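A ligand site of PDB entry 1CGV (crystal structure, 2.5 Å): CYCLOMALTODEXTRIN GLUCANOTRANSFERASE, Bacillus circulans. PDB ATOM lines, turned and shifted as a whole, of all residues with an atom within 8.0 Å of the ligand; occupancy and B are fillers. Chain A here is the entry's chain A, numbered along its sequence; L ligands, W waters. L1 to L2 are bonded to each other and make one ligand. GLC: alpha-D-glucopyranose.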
ATOM      1  N   TYR A 301     -10.520  10.370  30.331  1.00  0.00           N
ATOM      2  CA  TYR A 301      -9.394  10.739  31.144  1.00  0.00           C
ATOM      3  C   TYR A 301      -9.684  10.526  32.607  1.00  0.00           C
ATOM      4  O   TYR A 301      -8.785  10.185  33.388  1.00  0.00           O
ATOM      5  CB  TYR A 301      -8.924  12.173  30.815  1.00  0.00           C
ATOM      6  CG  TYR A 301      -8.406  12.241  29.398  1.00  0.00           C
ATOM      7  CD1 TYR A 301      -7.122  11.774  29.125  1.00  0.00           C
ATOM      8  CD2 TYR A 301      -9.190  12.695  28.335  1.00  0.00           C
ATOM      9  CE1 TYR A 301      -6.594  11.792  27.830  1.00  0.00           C
ATOM     10  CE2 TYR A 301      -8.678  12.720  27.040  1.00  0.00           C
ATOM     11  CZ  TYR A 301      -7.382  12.284  26.783  1.00  0.00           C
ATOM     12  OH  TYR A 301      -6.890  12.353  25.504  1.00  0.00           O
ATOM     13  N   LYS A 304      -9.659   6.840  33.374  1.00  0.00           N
ATOM     14  CA  LYS A 304      -8.275   6.485  33.449  1.00  0.00           C
ATOM     15  C   LYS A 304      -7.707   6.848  34.793  1.00  0.00           C
ATOM     16  O   LYS A 304      -7.022   6.071  35.425  1.00  0.00           O
ATOM     17  CB  LYS A 304      -7.419   7.141  32.397  1.00  0.00           C
ATOM     18  CG  LYS A 304      -5.957   6.817  32.606  1.00  0.00           C
ATOM     19  CD  LYS A 304      -5.040   7.325  31.500  1.00  0.00           C
ATOM     20  CE  LYS A 304      -3.790   8.072  31.954  1.00  0.00           C
ATOM     21  NZ  LYS A 304      -2.570   7.748  31.175  1.00  0.00           N
ATOM     22  N   GLN A 410      -3.605  -1.406  32.052  1.00  0.00           N
ATOM     23  CA  GLN A 410      -2.782  -0.384  31.457  1.00  0.00           C
ATOM     24  C   GLN A 410      -3.440   0.271  30.306  1.00  0.00           C
ATOM     25  O   GLN A 410      -3.903  -0.420  29.395  1.00  0.00           O
ATOM     26  CB  GLN A 410      -1.514  -1.045  30.942  1.00  0.00           C
ATOM     27  CG  GLN A 410      -0.366  -0.063  30.857  1.00  0.00           C
ATOM     28  CD  GLN A 410       0.710  -0.558  29.938  1.00  0.00           C
ATOM     29  OE1 GLN A 410       1.411   0.258  29.336  1.00  0.00           O
ATOM     30  NE2 GLN A 410       0.828  -1.874  29.811  1.00  0.00           N
ATOM     31  N   GLU A 411      -3.463   1.605  30.315  1.00  0.00           N
ATOM     32  CA  GLU A 411      -4.037   2.335  29.214  1.00  0.00           C
ATOM     33  C   GLU A 411      -3.156   2.208  27.963  1.00  0.00           C
ATOM     34  O   GLU A 411      -1.953   2.448  28.047  1.00  0.00           O
ATOM     35  CB  GLU A 411      -4.217   3.849  29.546  1.00  0.00           C
ATOM     36  CG  GLU A 411      -4.544   4.737  28.336  1.00  0.00           C
ATOM     37  CD  GLU A 411      -3.337   5.339  27.690  1.00  0.00           C
ATOM     38  OE1 GLU A 411      -2.468   6.047  28.239  1.00  0.00           O
ATOM     39  OE2 GLU A 411      -3.332   5.169  26.428  1.00  0.00           O
ATOM     40  N   ARG A 412      -3.710   1.854  26.813  1.00  0.00           N
ATOM     41  CA  ARG A 412      -2.846   1.832  25.640  1.00  0.00           C
ATOM     42  C   ARG A 412      -3.196   2.891  24.596  1.00  0.00           C
ATOM     43  O   ARG A 412      -2.397   3.260  23.758  1.00  0.00           O
ATOM     44  CB  ARG A 412      -2.500   0.515  24.950  1.00  0.00           C
ATOM     45  CG  ARG A 412      -2.777  -0.704  25.760  1.00  0.00           C
ATOM     46  CD  ARG A 412      -1.541  -1.333  26.394  1.00  0.00           C
ATOM     47  NE  ARG A 412      -0.238  -0.945  25.902  1.00  0.00           N
ATOM     48  CZ  ARG A 412       0.838  -1.754  25.945  1.00  0.00           C
ATOM     49  NH1 ARG A 412       0.833  -3.000  26.410  1.00  0.00           N
ATOM     50  NH2 ARG A 412       1.995  -1.325  25.484  1.00  0.00           N
ATOM     51  N   TRP A 413      -4.422   3.340  24.658  1.00  0.00           N
ATOM     52  CA  TRP A 413      -4.852   4.356  23.741  1.00  0.00           C
ATOM     53  C   TRP A 413      -5.984   5.136  24.368  1.00  0.00           C
ATOM     54  O   TRP A 413      -6.837   4.604  25.077  1.00  0.00           O
ATOM     55  CB  TRP A 413      -5.190   3.737  22.385  1.00  0.00           C
ATOM     56  CG  TRP A 413      -5.073   4.625  21.202  1.00  0.00           C
ATOM     57  CD1 TRP A 413      -4.076   4.603  20.299  1.00  0.00           C
ATOM     58  CD2 TRP A 413      -6.040   5.573  20.708  1.00  0.00           C
ATOM     59  NE1 TRP A 413      -4.329   5.480  19.293  1.00  0.00           N
ATOM     60  CE2 TRP A 413      -5.528   6.103  19.512  1.00  0.00           C
ATOM     61  CE3 TRP A 413      -7.266   6.052  21.188  1.00  0.00           C
ATOM     62  CZ2 TRP A 413      -6.204   7.078  18.785  1.00  0.00           C
ATOM     63  CZ3 TRP A 413      -7.928   7.017  20.475  1.00  0.00           C
ATOM     64  CH2 TRP A 413      -7.412   7.539  19.286  1.00  0.00           C
ATOM     65  N   ILE A 414      -5.976   6.430  24.135  1.00  0.00           N
ATOM     66  CA  ILE A 414      -7.026   7.162  24.759  1.00  0.00           C
ATOM     67  C   ILE A 414      -7.346   8.542  24.183  1.00  0.00           C
ATOM     68  O   ILE A 414      -6.488   9.270  23.707  1.00  0.00           O
ATOM     69  CB  ILE A 414      -6.724   7.286  26.255  1.00  0.00           C
ATOM     70  CG1 ILE A 414      -7.907   7.933  26.982  1.00  0.00           C
ATOM     71  CG2 ILE A 414      -5.486   8.174  26.465  1.00  0.00           C
ATOM     72  CD1 ILE A 414      -7.576   8.325  28.411  1.00  0.00           C
ATOM     73  N   ASN A 415      -8.589   8.915  24.311  1.00  0.00           N
ATOM     74  CA  ASN A 415      -9.066  10.229  23.928  1.00  0.00           C
ATOM     75  C   ASN A 415     -10.259  10.579  24.812  1.00  0.00           C
ATOM     76  O   ASN A 415     -10.522   9.904  25.799  1.00  0.00           O
ATOM     77  CB  ASN A 415      -9.188  10.544  22.432  1.00  0.00           C
ATOM     78  CG  ASN A 415     -10.458  10.046  21.776  1.00  0.00           C
ATOM     79  OD1 ASN A 415     -11.433   9.681  22.442  1.00  0.00           O
ATOM     80  ND2 ASN A 415     -10.420  10.008  20.442  1.00  0.00           N
ATOM     81  N   ASN A 416     -11.008  11.603  24.501  1.00  0.00           N
ATOM     82  CA  ASN A 416     -12.127  11.904  25.366  1.00  0.00           C
ATOM     83  C   ASN A 416     -13.154  10.819  25.475  1.00  0.00           C
ATOM     84  O   ASN A 416     -13.777  10.674  26.522  1.00  0.00           O
ATOM     85  CB  ASN A 416     -12.945  13.045  24.762  1.00  0.00           C
ATOM     86  CG  ASN A 416     -12.309  14.379  24.954  1.00  0.00           C
ATOM     87  OD1 ASN A 416     -12.717  15.366  24.333  1.00  0.00           O
ATOM     88  ND2 ASN A 416     -11.265  14.421  25.769  1.00  0.00           N
ATOM     89  N   VAL A 418     -12.762   7.502  23.778  1.00  0.00           N
ATOM     90  CA  VAL A 418     -12.324   6.166  23.600  1.00  0.00           C
ATOM     91  C   VAL A 418     -11.332   5.737  24.649  1.00  0.00           C
ATOM     92  O   VAL A 418     -10.483   6.517  25.059  1.00  0.00           O
ATOM     93  CB  VAL A 418     -11.568   6.034  22.277  1.00  0.00           C
ATOM     94  CG1 VAL A 418     -11.007   4.647  22.085  1.00  0.00           C
ATOM     95  CG2 VAL A 418     -12.420   6.436  21.097  1.00  0.00           C
ATOM     96  N   ILE A 420      -8.787   2.319  25.364  1.00  0.00           N
ATOM     97  CA  ILE A 420      -8.241   1.019  25.068  1.00  0.00           C
ATOM     98  C   ILE A 420      -7.300   0.604  26.180  1.00  0.00           C
ATOM     99  O   ILE A 420      -6.303   1.233  26.451  1.00  0.00           O
ATOM    100  CB  ILE A 420      -7.599   0.928  23.706  1.00  0.00           C
ATOM    101  CG1 ILE A 420      -8.584   1.441  22.657  1.00  0.00           C
ATOM    102  CG2 ILE A 420      -7.293  -0.531  23.409  1.00  0.00           C
ATOM    103  CD1 ILE A 420      -8.087   1.242  21.237  1.00  0.00           C
ATOM    104  N   SER A 443     -10.699   6.965  14.770  1.00  0.00           N
ATOM    105  CA  SER A 443      -9.566   6.477  13.983  1.00  0.00           C
ATOM    106  C   SER A 443      -8.435   6.085  14.880  1.00  0.00           C
ATOM    107  O   SER A 443      -7.710   6.931  15.412  1.00  0.00           O
ATOM    108  CB  SER A 443      -9.047   7.486  13.007  1.00  0.00           C
ATOM    109  OG  SER A 443      -9.369   6.991  11.751  1.00  0.00           O
ATOM    110  N   ILE A 444      -8.313   4.789  15.001  1.00  0.00           N
ATOM    111  CA  ILE A 444      -7.296   4.239  15.845  1.00  0.00           C
ATOM    112  C   ILE A 444      -6.007   3.888  15.147  1.00  0.00           C
ATOM    113  O   ILE A 444      -5.925   2.930  14.396  1.00  0.00           O
ATOM    114  CB  ILE A 444      -7.844   3.188  16.800  1.00  0.00           C
ATOM    115  CG1 ILE A 444      -8.558   3.974  17.893  1.00  0.00           C
ATOM    116  CG2 ILE A 444      -6.667   2.451  17.415  1.00  0.00           C
ATOM    117  CD1 ILE A 444      -9.946   3.504  18.222  1.00  0.00           C
ATOM    118  N   SER A 445      -4.997   4.712  15.403  1.00  0.00           N
ATOM    119  CA  SER A 445      -3.666   4.491  14.868  1.00  0.00           C
ATOM    120  C   SER A 445      -2.682   4.676  16.007  1.00  0.00           C
ATOM    121  O   SER A 445      -2.917   5.512  16.893  1.00  0.00           O
ATOM    122  CB  SER A 445      -3.241   5.310  13.664  1.00  0.00           C
ATOM    123  OG  SER A 445      -3.748   6.608  13.780  1.00  0.00           O
ATOM    124  N   GLY A 446      -1.609   3.857  15.951  1.00  0.00           N
ATOM    125  CA  GLY A 446      -0.540   3.873  16.960  1.00  0.00           C
ATOM    126  C   GLY A 446      -0.743   2.971  18.175  1.00  0.00           C
ATOM    127  O   GLY A 446      -0.011   3.075  19.178  1.00  0.00           O
ATOM    128  N   LEU A 447      -1.740   2.089  18.097  1.00  0.00           N
ATOM    129  CA  LEU A 447      -2.024   1.182  19.176  1.00  0.00           C
ATOM    130  C   LEU A 447      -0.935   0.119  19.279  1.00  0.00           C
ATOM    131  O   LEU A 447      -0.630  -0.584  18.317  1.00  0.00           O
ATOM    132  CB  LEU A 447      -3.403   0.526  18.930  1.00  0.00           C
ATOM    133  CG  LEU A 447      -3.684  -0.619  19.890  1.00  0.00           C
ATOM    134  CD1 LEU A 447      -3.873  -0.036  21.289  1.00  0.00           C
ATOM    135  CD2 LEU A 447      -4.917  -1.390  19.433  1.00  0.00           C
ATOM    136  N   VAL A 448      -0.342   0.009  20.446  1.00  0.00           N
ATOM    137  CA  VAL A 448       0.684  -0.989  20.670  1.00  0.00           C
ATOM    138  C   VAL A 448       0.210  -1.872  21.801  1.00  0.00           C
ATOM    139  O   VAL A 448      -0.320  -1.385  22.800  1.00  0.00           O
ATOM    140  CB  VAL A 448       2.007  -0.341  21.091  1.00  0.00           C
ATOM    141  CG1 VAL A 448       3.015  -1.398  21.473  1.00  0.00           C
ATOM    142  CG2 VAL A 448       2.587   0.546  20.009  1.00  0.00           C
ATOM    143  N   THR A 449       0.394  -3.176  21.670  1.00  0.00           N
ATOM    144  CA  THR A 449      -0.043  -4.080  22.719  1.00  0.00           C
ATOM    145  C   THR A 449       0.970  -5.158  23.001  1.00  0.00           C
ATOM    146  O   THR A 449       2.036  -5.264  22.400  1.00  0.00           O
ATOM    147  CB  THR A 449      -1.363  -4.783  22.328  1.00  0.00           C
ATOM    148  OG1 THR A 449      -1.084  -5.782  21.360  1.00  0.00           O
ATOM    149  CG2 THR A 449      -2.303  -3.782  21.696  1.00  0.00           C
ATOM    150  N   ALA A 476       2.433  -3.997  17.586  1.00  0.00           N
ATOM    151  CA  ALA A 476       1.794  -2.821  17.047  1.00  0.00           C
ATOM    152  C   ALA A 476       0.620  -3.221  16.170  1.00  0.00           C
ATOM    153  O   ALA A 476       0.776  -4.039  15.265  1.00  0.00           O
ATOM    154  CB  ALA A 476       2.805  -2.024  16.298  1.00  0.00           C
HETATM  155  C1  GLC L   1      -3.524   9.278  19.864  1.00  0.00           C
HETATM  156  C2  GLC L   1      -4.169   8.759  21.114  1.00  0.00           C
HETATM  157  C3  GLC L   1      -3.094   8.382  22.096  1.00  0.00           C
HETATM  158  C4  GLC L   1      -2.186   7.357  21.433  1.00  0.00           C
HETATM  159  C5  GLC L   1      -1.550   7.948  20.179  1.00  0.00           C
HETATM  160  C6  GLC L   1      -0.748   6.886  19.458  1.00  0.00           C
HETATM  161  O1  GLC L   1      -2.905  10.472  20.179  1.00  0.00           O
HETATM  162  O2  GLC L   1      -4.927   9.804  21.717  1.00  0.00           O
HETATM  163  O3  GLC L   1      -3.734   7.842  23.245  1.00  0.00           O
HETATM  164  O4  GLC L   1      -1.138   6.990  22.357  1.00  0.00           O
HETATM  165  O5  GLC L   1      -2.625   8.312  19.318  1.00  0.00           O
HETATM  166  O6  GLC L   1      -0.215   7.456  18.268  1.00  0.00           O
HETATM  167  C1  GLC L   2      -1.070   5.641  22.752  1.00  0.00           C
HETATM  168  C2  GLC L   2      -0.806   5.616  24.250  1.00  0.00           C
HETATM  169  C3  GLC L   2       0.568   6.196  24.468  1.00  0.00           C
HETATM  170  C4  GLC L   2       1.597   5.355  23.734  1.00  0.00           C
HETATM  171  C5  GLC L   2       1.265   5.364  22.254  1.00  0.00           C
HETATM  172  C6  GLC L   2       2.196   4.446  21.525  1.00  0.00           C
HETATM  173  O2  GLC L   2      -1.734   6.492  24.887  1.00  0.00           O
HETATM  174  O3  GLC L   2       0.927   6.303  25.842  1.00  0.00           O
HETATM  175  O4  GLC L   2       2.901   5.910  23.821  1.00  0.00           O
HETATM  176  O5  GLC L   2      -0.081   4.939  22.012  1.00  0.00           O
HETATM  177  O6  GLC L   2       2.356   4.855  20.165  1.00  0.00           O
HETATM  178  O   HOH W   1       0.411   3.364  26.947  1.00  0.00           O
HETATM  179  O   HOH W   2       1.266   2.000  24.525  1.00  0.00           O
HETATM  180  O   HOH W   3      -0.493   2.214  22.332  1.00  0.00           O
HETATM  181  O   HOH W   4      -4.626  11.343  24.546  1.00  0.00           O
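O2 of GLC L2 is in hydrogen-bond range of OE2 of Glu 411, at 2.6 Å. An oxygen (O3) of GLC L1 sits at hydrogen-bond distance from the backbone NH (N) of Ile 414, at 2.8 Å. O of Ile 414 sits at hydrogen-bond distance from O2 of GLC L1 (2.6 Å). The backbone carbonyl oxygen (O) of Arg 412 sits close to an oxygen (O2) of GLC L2 (3.5 Å). The backbone carbonyl oxygen (O) of Gly 446 is in hydrogen-bond range of an oxygen (O6) of GLC L2, at 3.1 Å. NE1 of Trp 413 lies within hydrogen-bond range of O5 of GLC L1, at 3.3 Å.
The side-chain carboxylate (OE2) of Glu 411 is in hydrogen-bond range of the backbone NH (N) of Trp 413, 2.8 Å away. The side-chain carboxylate (OE1) of Glu 411 lies within salt-bridge range of the side-chain amino group (NZ) of Lys 304 (3.4 Å). NE of Arg 412 is in hydrogen-bond range of O of Val 448. O of Ile 420 sits at hydrogen-bond distance from N of Arg 412, 2.7 Å away. The indole nitrogen (NE1) of Trp 413 sits at hydrogen-bond distance from the backbone carbonyl oxygen (O) of Ser 445. N of Ile 420 lies within hydrogen-bond range of O of Trp 413 (3.0 Å).
Residues that only touch the ligand: Ser 445 (3.6 Å). Hydrophobic or aromatic side chains that line the ligand: Trp 413 and Ile 414.
Water W1 lies within hydrogen-bond range of the backbone carbonyl oxygen (O) of Glu 411 (2.8 Å) and an oxygen (O3) of GLC L2 (3.2 Å). Water W4 lies within hydrogen-bond range of the side-chain hydroxyl of Tyr 301 (2.7 Å), the backbone carbonyl oxygen of Ile 414 (2.9 Å) and an oxygen (O2) of GLC L1 (3.2 Å).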
